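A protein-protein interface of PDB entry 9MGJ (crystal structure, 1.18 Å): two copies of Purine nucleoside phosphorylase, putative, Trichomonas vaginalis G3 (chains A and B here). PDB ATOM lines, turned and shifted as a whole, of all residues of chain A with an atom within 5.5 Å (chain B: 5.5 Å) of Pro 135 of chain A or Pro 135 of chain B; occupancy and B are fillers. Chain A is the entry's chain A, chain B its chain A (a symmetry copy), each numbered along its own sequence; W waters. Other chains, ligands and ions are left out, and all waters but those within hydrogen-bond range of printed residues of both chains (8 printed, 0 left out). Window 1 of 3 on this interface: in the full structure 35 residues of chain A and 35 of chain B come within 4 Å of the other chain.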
ATOM      1  N   ALA A 117       7.750 -15.843  -9.271  1.00  0.00           N
ATOM      2  CA  ALA A 117       8.318 -15.841  -7.927  1.00  0.00           C
ATOM      3  C   ALA A 117       9.350 -14.726  -7.899  1.00  0.00           C
ATOM      4  O   ALA A 117       9.840 -14.298  -8.944  1.00  0.00           O
ATOM      5  CB  ALA A 117       8.998 -17.168  -7.569  1.00  0.00           C
ATOM      6  N   SER A 118       9.735 -14.304  -6.688  1.00  0.00           N
ATOM      7  CA  SER A 118      10.632 -13.161  -6.527  1.00  0.00           C
ATOM      8  C   SER A 118      11.705 -13.456  -5.496  1.00  0.00           C
ATOM      9  O   SER A 118      11.390 -13.870  -4.380  1.00  0.00           O
ATOM     10  CB  SER A 118       9.863 -11.931  -6.059  1.00  0.00           C
ATOM     11  OG  SER A 118       8.855 -11.703  -7.001  1.00  0.00           O
ATOM     12  N   GLY A 119      12.954 -13.230  -5.871  1.00  0.00           N
ATOM     13  CA  GLY A 119      14.048 -13.271  -4.918  1.00  0.00           C
ATOM     14  C   GLY A 119      14.142 -11.944  -4.185  1.00  0.00           C
ATOM     15  O   GLY A 119      13.408 -11.000  -4.468  1.00  0.00           O
ATOM     16  N   THR A 120      15.044 -11.863  -3.212  1.00  0.00           N
ATOM     17  CA  THR A 120      15.188 -10.626  -2.448  1.00  0.00           C
ATOM     18  C   THR A 120      16.486 -10.628  -1.668  1.00  0.00           C
ATOM     19  O   THR A 120      17.067 -11.680  -1.370  1.00  0.00           O
ATOM     20  CB  THR A 120      13.986 -10.418  -1.522  1.00  0.00           C
ATOM     21  OG1 THR A 120      14.068  -9.117  -0.927  1.00  0.00           O
ATOM     22  CG2 THR A 120      13.905 -11.435  -0.414  1.00  0.00           C
ATOM     23  N   ASP A 133      15.222 -20.674   3.327  1.00  0.00           N
ATOM     24  CA  ASP A 133      14.793 -20.062   2.067  1.00  0.00           C
ATOM     25  C   ASP A 133      13.302 -20.301   1.852  1.00  0.00           C
ATOM     26  O   ASP A 133      12.868 -21.454   1.683  1.00  0.00           O
ATOM     27  CB  ASP A 133      15.535 -20.615   0.853  1.00  0.00           C
ATOM     28  CG  ASP A 133      16.989 -20.191   0.762  1.00  0.00           C
ATOM     29  OD1 ASP A 133      17.509 -19.618   1.719  1.00  0.00           O
ATOM     30  OD2 ASP A 133      17.611 -20.449  -0.306  1.00  0.00           O
ATOM     31  N   PHE A 134      12.548 -19.211   1.813  1.00  0.00           N
ATOM     32  CA  PHE A 134      11.098 -19.207   1.639  1.00  0.00           C
ATOM     33  C   PHE A 134      10.849 -18.475   0.328  1.00  0.00           C
ATOM     34  O   PHE A 134      10.988 -17.243   0.278  1.00  0.00           O
ATOM     35  CB  PHE A 134      10.506 -18.453   2.828  1.00  0.00           C
ATOM     36  CG  PHE A 134       8.981 -18.264   2.808  1.00  0.00           C
ATOM     37  CD1 PHE A 134       8.172 -18.558   1.713  1.00  0.00           C
ATOM     38  CD2 PHE A 134       8.382 -17.754   3.945  1.00  0.00           C
ATOM     39  CE1 PHE A 134       6.795 -18.326   1.773  1.00  0.00           C
ATOM     40  CE2 PHE A 134       7.016 -17.514   4.000  1.00  0.00           C
ATOM     41  CZ  PHE A 134       6.224 -17.809   2.922  1.00  0.00           C
ATOM     42  N   PRO A 135      10.490 -19.158  -0.761  1.00  0.00           N
ATOM     43  CA  PRO A 135      10.296 -18.451  -2.038  1.00  0.00           C
ATOM     44  C   PRO A 135       9.023 -17.627  -1.997  1.00  0.00           C
ATOM     45  O   PRO A 135       7.948 -18.144  -1.678  1.00  0.00           O
ATOM     46  CB  PRO A 135      10.183 -19.590  -3.055  1.00  0.00           C
ATOM     47  CG  PRO A 135       9.596 -20.714  -2.272  1.00  0.00           C
ATOM     48  CD  PRO A 135      10.216 -20.594  -0.883  1.00  0.00           C
ATOM     49  N   ALA A 136       9.161 -16.342  -2.306  1.00  0.00           N
ATOM     50  CA  ALA A 136       8.006 -15.484  -2.505  1.00  0.00           C
ATOM     51  C   ALA A 136       7.385 -15.866  -3.844  1.00  0.00           C
ATOM     52  O   ALA A 136       7.975 -15.610  -4.891  1.00  0.00           O
ATOM     53  CB  ALA A 136       8.473 -14.034  -2.497  1.00  0.00           C
ATOM     54  N   THR A 137       6.233 -16.519  -3.806  1.00  0.00           N
ATOM     55  CA  THR A 137       5.699 -17.226  -4.962  1.00  0.00           C
ATOM     56  C   THR A 137       4.311 -16.683  -5.288  1.00  0.00           C
ATOM     57  O   THR A 137       3.422 -16.663  -4.430  1.00  0.00           O
ATOM     58  CB  THR A 137       5.645 -18.743  -4.673  1.00  0.00           C
ATOM     59  OG1 THR A 137       6.926 -19.198  -4.221  1.00  0.00           O
ATOM     60  CG2 THR A 137       5.288 -19.527  -5.920  1.00  0.00           C
ATOM     61  N   LYS A 161      11.061 -14.997 -13.101  1.00  0.00           N
ATOM     62  CA  LYS A 161      11.419 -14.525 -11.768  1.00  0.00           C
ATOM     63  C   LYS A 161      11.678 -13.029 -11.728  1.00  0.00           C
ATOM     64  O   LYS A 161      12.312 -12.466 -12.621  1.00  0.00           O
ATOM     65  CB  LYS A 161      12.709 -15.206 -11.301  1.00  0.00           C
ATOM     66  CG  LYS A 161      12.624 -16.722 -11.120  1.00  0.00           C
ATOM     67  CD  LYS A 161      13.941 -17.284 -10.607  1.00  0.00           C
ATOM     68  CE  LYS A 161      15.102 -17.015 -11.544  1.00  0.00           C
ATOM     69  NZ  LYS A 161      14.996 -17.662 -12.862  1.00  0.00           N
ATOM     70  N   ALA A 162      11.264 -12.408 -10.632  1.00  0.00           N
ATOM     71  CA  ALA A 162      11.666 -11.058 -10.270  1.00  0.00           C
ATOM     72  C   ALA A 162      12.677 -11.121  -9.135  1.00  0.00           C
ATOM     73  O   ALA A 162      12.874 -12.158  -8.499  1.00  0.00           O
ATOM     74  CB  ALA A 162      10.458 -10.251  -9.814  1.00  0.00           C
ATOM     75  N   PHE A 184      16.782 -13.904 -14.153  1.00  0.00           N
ATOM     76  CA  PHE A 184      15.784 -13.038 -13.545  1.00  0.00           C
ATOM     77  C   PHE A 184      15.364 -12.005 -14.581  1.00  0.00           C
ATOM     78  O   PHE A 184      16.217 -11.374 -15.218  1.00  0.00           O
ATOM     79  CB  PHE A 184      16.383 -12.348 -12.317  1.00  0.00           C
ATOM     80  CG  PHE A 184      16.516 -13.261 -11.105  1.00  0.00           C
ATOM     81  CD1 PHE A 184      17.568 -14.163 -10.988  1.00  0.00           C
ATOM     82  CD2 PHE A 184      15.566 -13.226 -10.095  1.00  0.00           C
ATOM     83  CE1 PHE A 184      17.665 -14.986  -9.883  1.00  0.00           C
ATOM     84  CE2 PHE A 184      15.656 -14.049  -9.001  1.00  0.00           C
ATOM     85  CZ  PHE A 184      16.710 -14.939  -8.898  1.00  0.00           C
ATOM     86  N   PRO A 196       4.386 -13.669   0.456  1.00  0.00           N
ATOM     87  CA  PRO A 196       4.280 -14.415   1.721  1.00  0.00           C
ATOM     88  C   PRO A 196       3.161 -13.936   2.613  1.00  0.00           C
ATOM     89  O   PRO A 196       2.622 -14.726   3.399  1.00  0.00           O
ATOM     90  CB  PRO A 196       5.658 -14.227   2.357  1.00  0.00           C
ATOM     91  CG  PRO A 196       6.563 -13.993   1.168  1.00  0.00           C
ATOM     92  CD  PRO A 196       5.738 -13.108   0.281  1.00  0.00           C
ATOM     93  N   ASP A 199       0.140 -15.655   1.412  1.00  0.00           N
ATOM     94  CA  ASP A 199       0.171 -17.022   1.928  1.00  0.00           C
ATOM     95  C   ASP A 199      -0.332 -17.072   3.367  1.00  0.00           C
ATOM     96  O   ASP A 199      -1.127 -17.937   3.726  1.00  0.00           O
ATOM     97  CB  ASP A 199       1.586 -17.598   1.906  1.00  0.00           C
ATOM     98  CG  ASP A 199       2.121 -17.885   0.528  1.00  0.00           C
ATOM     99  OD1 ASP A 199       1.337 -18.068  -0.415  1.00  0.00           O
ATOM    100  OD2 ASP A 199       3.365 -17.992   0.408  1.00  0.00           O
ATOM    101  N   ALA B 117       7.201 -23.407  -6.962  1.00  0.00           N
ATOM    102  CA  ALA B 117       8.501 -22.980  -6.456  1.00  0.00           C
ATOM    103  C   ALA B 117       8.764 -23.798  -5.202  1.00  0.00           C
ATOM    104  O   ALA B 117       7.835 -24.327  -4.592  1.00  0.00           O
ATOM    105  CB  ALA B 117       8.539 -21.488  -6.103  1.00  0.00           C
ATOM    106  N   SER B 118      10.032 -23.840  -4.775  1.00  0.00           N
ATOM    107  CA  SER B 118      10.433 -24.684  -3.652  1.00  0.00           C
ATOM    108  C   SER B 118      11.353 -23.931  -2.710  1.00  0.00           C
ATOM    109  O   SER B 118      12.351 -23.360  -3.149  1.00  0.00           O
ATOM    110  CB  SER B 118      11.179 -25.919  -4.142  1.00  0.00           C
ATOM    111  OG  SER B 118      10.330 -26.574  -5.039  1.00  0.00           O
ATOM    112  N   GLY B 119      11.018 -23.947  -1.429  1.00  0.00           N
ATOM    113  CA  GLY B 119      11.919 -23.448  -0.406  1.00  0.00           C
ATOM    114  C   GLY B 119      12.932 -24.521  -0.044  1.00  0.00           C
ATOM    115  O   GLY B 119      12.881 -25.645  -0.537  1.00  0.00           O
ATOM    116  N   THR B 120      13.883 -24.176   0.819  1.00  0.00           N
ATOM    117  CA  THR B 120      14.904 -25.145   1.208  1.00  0.00           C
ATOM    118  C   THR B 120      15.642 -24.675   2.445  1.00  0.00           C
ATOM    119  O   THR B 120      15.685 -23.480   2.764  1.00  0.00           O
ATOM    120  CB  THR B 120      15.873 -25.406   0.051  1.00  0.00           C
ATOM    121  OG1 THR B 120      16.745 -26.488   0.401  1.00  0.00           O
ATOM    122  CG2 THR B 120      16.724 -24.212  -0.295  1.00  0.00           C
ATOM    123  N   ASP B 133      18.257 -14.319  -1.213  1.00  0.00           N
ATOM    124  CA  ASP B 133      17.176 -15.278  -1.449  1.00  0.00           C
ATOM    125  C   ASP B 133      16.937 -15.436  -2.947  1.00  0.00           C
ATOM    126  O   ASP B 133      16.518 -14.479  -3.622  1.00  0.00           O
ATOM    127  CB  ASP B 133      15.855 -14.858  -0.807  1.00  0.00           C
ATOM    128  CG  ASP B 133      15.839 -14.951   0.708  1.00  0.00           C
ATOM    129  OD1 ASP B 133      16.892 -15.162   1.308  1.00  0.00           O
ATOM    130  OD2 ASP B 133      14.730 -14.805   1.294  1.00  0.00           O
ATOM    131  N   PHE B 134      17.157 -16.649  -3.436  1.00  0.00           N
ATOM    132  CA  PHE B 134      17.012 -17.019  -4.841  1.00  0.00           C
ATOM    133  C   PHE B 134      15.904 -18.063  -4.873  1.00  0.00           C
ATOM    134  O   PHE B 134      16.133 -19.211  -4.460  1.00  0.00           O
ATOM    135  CB  PHE B 134      18.350 -17.602  -5.291  1.00  0.00           C
ATOM    136  CG  PHE B 134      18.398 -18.131  -6.734  1.00  0.00           C
ATOM    137  CD1 PHE B 134      17.279 -18.279  -7.549  1.00  0.00           C
ATOM    138  CD2 PHE B 134      19.631 -18.495  -7.243  1.00  0.00           C
ATOM    139  CE1 PHE B 134      17.413 -18.797  -8.840  1.00  0.00           C
ATOM    140  CE2 PHE B 134      19.761 -19.018  -8.522  1.00  0.00           C
ATOM    141  CZ  PHE B 134      18.657 -19.159  -9.322  1.00  0.00           C
ATOM    142  N   PRO B 135      14.695 -17.741  -5.337  1.00  0.00           N
ATOM    143  CA  PRO B 135      13.615 -18.740  -5.323  1.00  0.00           C
ATOM    144  C   PRO B 135      13.862 -19.800  -6.380  1.00  0.00           C
ATOM    145  O   PRO B 135      14.074 -19.482  -7.554  1.00  0.00           O
ATOM    146  CB  PRO B 135      12.368 -17.914  -5.651  1.00  0.00           C
ATOM    147  CG  PRO B 135      12.887 -16.806  -6.503  1.00  0.00           C
ATOM    148  CD  PRO B 135      14.257 -16.468  -5.921  1.00  0.00           C
ATOM    149  N   ALA B 136      13.849 -21.057  -5.947  1.00  0.00           N
ATOM    150  CA  ALA B 136      13.868 -22.175  -6.872  1.00  0.00           C
ATOM    151  C   ALA B 136      12.488 -22.254  -7.515  1.00  0.00           C
ATOM    152  O   ALA B 136      11.516 -22.597  -6.846  1.00  0.00           O
ATOM    153  CB  ALA B 136      14.197 -23.443  -6.093  1.00  0.00           C
ATOM    154  N   THR B 137      12.397 -21.886  -8.784  1.00  0.00           N
ATOM    155  CA  THR B 137      11.119 -21.595  -9.422  1.00  0.00           C
ATOM    156  C   THR B 137      10.947 -22.497 -10.640  1.00  0.00           C
ATOM    157  O   THR B 137      11.802 -22.525 -11.532  1.00  0.00           O
ATOM    158  CB  THR B 137      11.059 -20.105  -9.824  1.00  0.00           C
ATOM    159  OG1 THR B 137      11.374 -19.282  -8.695  1.00  0.00           O
ATOM    160  CG2 THR B 137       9.672 -19.721 -10.303  1.00  0.00           C
ATOM    161  N   LYS B 161       3.608 -24.319  -3.411  1.00  0.00           N
ATOM    162  CA  LYS B 161       5.007 -24.387  -3.004  1.00  0.00           C
ATOM    163  C   LYS B 161       5.380 -25.737  -2.419  1.00  0.00           C
ATOM    164  O   LYS B 161       4.627 -26.328  -1.644  1.00  0.00           O
ATOM    165  CB  LYS B 161       5.287 -23.345  -1.917  1.00  0.00           C
ATOM    166  CG  LYS B 161       5.122 -21.886  -2.345  1.00  0.00           C
ATOM    167  CD  LYS B 161       5.472 -20.941  -1.206  1.00  0.00           C
ATOM    168  CE  LYS B 161       4.602 -21.143   0.018  1.00  0.00           C
ATOM    169  NZ  LYS B 161       3.174 -20.849  -0.183  1.00  0.00           N
ATOM    170  N   ALA B 162       6.595 -26.174  -2.722  1.00  0.00           N
ATOM    171  CA  ALA B 162       7.245 -27.282  -2.041  1.00  0.00           C
ATOM    172  C   ALA B 162       8.320 -26.739  -1.110  1.00  0.00           C
ATOM    173  O   ALA B 162       8.702 -25.570  -1.173  1.00  0.00           O
ATOM    174  CB  ALA B 162       7.891 -28.218  -3.053  1.00  0.00           C
ATOM    175  N   PHE B 184       2.737 -24.297   2.444  1.00  0.00           N
ATOM    176  CA  PHE B 184       3.541 -25.207   1.644  1.00  0.00           C
ATOM    177  C   PHE B 184       2.772 -26.514   1.502  1.00  0.00           C
ATOM    178  O   PHE B 184       2.280 -27.061   2.497  1.00  0.00           O
ATOM    179  CB  PHE B 184       4.883 -25.451   2.338  1.00  0.00           C
ATOM    180  CG  PHE B 184       5.855 -24.284   2.219  1.00  0.00           C
ATOM    181  CD1 PHE B 184       5.747 -23.165   3.039  1.00  0.00           C
ATOM    182  CD2 PHE B 184       6.862 -24.307   1.266  1.00  0.00           C
ATOM    183  CE1 PHE B 184       6.636 -22.115   2.909  1.00  0.00           C
ATOM    184  CE2 PHE B 184       7.740 -23.261   1.131  1.00  0.00           C
ATOM    185  CZ  PHE B 184       7.621 -22.155   1.954  1.00  0.00           C
ATOM    186  N   PRO B 196      17.222 -24.051 -10.097  1.00  0.00           N
ATOM    187  CA  PRO B 196      18.287 -23.085 -10.412  1.00  0.00           C
ATOM    188  C   PRO B 196      19.283 -23.592 -11.427  1.00  0.00           C
ATOM    189  O   PRO B 196      19.878 -22.790 -12.156  1.00  0.00           O
ATOM    190  CB  PRO B 196      18.926 -22.810  -9.051  1.00  0.00           C
ATOM    191  CG  PRO B 196      17.806 -23.093  -8.075  1.00  0.00           C
ATOM    192  CD  PRO B 196      17.156 -24.318  -8.648  1.00  0.00           C
ATOM    193  N   ASP B 199      17.773 -22.914 -14.711  1.00  0.00           N
ATOM    194  CA  ASP B 199      17.967 -21.496 -15.005  1.00  0.00           C
ATOM    195  C   ASP B 199      19.365 -21.240 -15.558  1.00  0.00           C
ATOM    196  O   ASP B 199      19.532 -20.519 -16.538  1.00  0.00           O
ATOM    197  CB  ASP B 199      17.792 -20.636 -13.755  1.00  0.00           C
ATOM    198  CG  ASP B 199      16.376 -20.550 -13.250  1.00  0.00           C
ATOM    199  OD1 ASP B 199      15.429 -20.765 -14.021  1.00  0.00           O
ATOM    200  OD2 ASP B 199      16.214 -20.194 -12.057  1.00  0.00           O
HETATM  201  O   HOH W   1      18.678 -18.451  -1.888  1.00  0.00           O
HETATM  202  O   HOH W   2      13.624 -16.812   2.837  1.00  0.00           O
HETATM  203  O   HOH W   3      12.324 -14.901  -0.049  1.00  0.00           O
HETATM  204  O   HOH W   4      17.931 -12.235   1.847  1.00  0.00           O
HETATM  205  O   HOH W   5      16.322 -21.202  -2.623  1.00  0.00           O
HETATM  206  O   HOH W   6      18.679 -22.038   3.367  1.00  0.00           O
HETATM  207  O   HOH W   7       2.636 -18.683  -2.668  1.00  0.00           O
HETATM  208  O   HOH W   8      13.074 -20.393 -12.813  1.00  0.00           O
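Water W8 lies within hydrogen-bond range of OD1 of Asp 199 of chain B (2.7 Å), O of Thr 137 of chain B (2.8 Å) and NZ of Lys 161 of chain A (3.3 Å).
Water W7 lies within hydrogen-bond range of the side-chain carboxylate of Asp 199 of chain A (2.7 Å), the backbone carbonyl oxygen of Thr 137 of chain A (2.8 Å) and the side-chain amino group of Lys 161 of chain B (3.3 Å).
Water W3 bridges the backbone carbonyl oxygen (O) of Phe 134 of chain A (2.7 Å) and the side-chain carboxylate (OD2) of Asp 133 of chain B (2.8 Å).
Water W5 lies within hydrogen-bond range of the backbone carbonyl oxygen (O) of Phe 134 of chain B (2.7 Å) and the side-chain carboxylate (OD2) of Asp 133 of chain A (2.8 Å).
Water W1 bridges OD2 of Asp 133 of chain A (2.8 Å) and N of Phe 134 of chain B (2.8 Å).
Water W6 lies within hydrogen-bond range of OD1 of Asp 133 of chain A (3.2 Å) and O of Thr 120 of chain B (3.4 Å).
The backbone NH (N) of Ala 162 of chain A sits at hydrogen-bond distance from the backbone carbonyl oxygen (O) of Ala 117 of chain A, 2.9 Å away.
The backbone carbonyl oxygen of Ala 136 of chain A lies within hydrogen-bond range of the backbone NH of Ser 118 of chain A.
The backbone carbonyl oxygen of Pro 135 of chain A sits at hydrogen-bond distance from the side-chain hydroxyl of Thr 137 of chain A, 2.9 Å away.
The backbone carbonyl oxygen (O) of Ala 117 of chain B lies within hydrogen-bond range of the backbone NH (N) of Ala 162 of chain B (2.9 Å).
N of Gly 119 of chain B is in hydrogen-bond range of O of Ala 162 of chain B, 2.8 Å away.
The backbone carbonyl oxygen of Pro 135 of chain B is in hydrogen-bond range of the side-chain hydroxyl of Thr 137 of chain B (2.9 Å).
Of the printed residues of chain B, Pro 135 of chain A touches Ala 117, Ser 118, Gly 119, Pro 135 and Lys 161.
Printed residues of chain A within 4 Å of Pro 135 of chain B: Ala 117 (3.9 Å), Ser 118 (3.7 Å), Gly 119 (3.4 Å), Pro 135 (3.8 Å) and Lys 161 (3.8 Å).
Of the printed residues of chain A, Phe 184 of chain B touches Phe 134.
Of the printed residues of chain B, Ser 118 of chain A touches Pro 135.
Printed residues of chain A within 4 Å of Gly 119 of chain B: Asp 133 and Pro 135.
The nearest printed residue of chain A that does not touch Pro 135 of chain B is Phe 184 of chain A (4.1 Å).
The nearest printed residue of chain B that does not touch Thr 120 of chain A is Phe 134 of chain B (5.2 Å).
Hydrophobic or aromatic side chains of chain A that line the printed part of chain B: Ala 117, Phe 134, Pro 135 and Phe 184.
Of the 14 printed residues of chain B, 11 touch a printed residue of chain A.
Hydrophobic or aromatic side chains of chain B that line the printed part of chain A: Ala 117, Phe 134, Pro 135 and Phe 184.
Among the printed residues, Asp or Glu carboxylates within 4 Å of a Lys or Arg side-chain nitrogen of the other chain: Lys 161 of chain A with Asp 199 of chain B and Asp 199 of chain A with Lys 161 of chain B.
Ala 117 of chain A touches Thr 137 of chain B, and with the chains exchanged Thr 137 of chain A touches Ala 117 of chain B.
Gly 119 of chain A touches Pro 135 of chain B, and with the chains exchanged Pro 135 of chain A touches Gly 119 of chain B.
Phe 134 of chain A touches Lys 161 of chain B, and with the chains exchanged Lys 161 of chain A touches Phe 134 of chain B.
Lys 161 of chain A touches Asp 199 of chain B, and with the chains exchanged Asp 199 of chain A touches Lys 161 of chain B.
14 positions are printed for both chains.
Of the 23 pairs that touch across the chains among the printed residues, 23 have their exchanged pair printed and touching as well.
The backbone carbonyl oxygen (O) of Thr 120 of chain A is in hydrogen-bond range of the backbone NH (N) of Asp 133 of chain B, at 2.9 Å.
The backbone carbonyl oxygen (O) of Thr 120 of chain B sits at hydrogen-bond distance from the backbone NH (N) of Asp 133 of chain A (2.9 Å).
The side-chain amino group (NZ) of Lys 161 of chain A is in salt-bridge range of the side-chain carboxylate (OD2) of Asp 199 of chain B (2.9 Å).
NZ of Lys 161 of chain B lies within salt-bridge range of OD2 of Asp 199 of chain A.
Among the printed residues, pairs that only touch across the chains: Ala 117 of chain A with Pro 135 of chain B (3.9 Å), Ala 117 of chain A with Thr 137 of chain B (3.4 Å), Ser 118 of chain A with Pro 135 of chain B (3.7 Å), Gly 119 of chain A with Asp 133 of chain B (3.0 Å), Gly 119 of chain A with Pro 135 of chain B (3.4 Å), Asp 133 of chain A with Gly 119 of chain B (3.0 Å), Phe 134 of chain A with Lys 161 of chain B (3.98 Å), Phe 134 of chain A with Phe 184 of chain B (3.6 Å), Pro 135 of chain A with Ala 117 of chain B (3.9 Å), Pro 135 of chain A with Ser 118 of chain B (3.7 Å), Pro 135 of chain A with Gly 119 of chain B (3.4 Å), Pro 135 of chain A with Pro 135 of chain B (3.8 Å), Pro 135 of chain A with Lys 161 of chain B (3.8 Å), Thr 137 of chain A with Ala 117 of chain B (3.4 Å), Thr 137 of chain A with Lys 161 of chain B (3.7 Å), Lys 161 of chain A with Phe 134 of chain B (3.98 Å), Lys 161 of chain A with Pro 135 of chain B (3.8 Å), Lys 161 of chain A with Thr 137 of chain B (3.7 Å) and Phe 184 of chain A with Phe 134 of chain B (3.6 Å).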
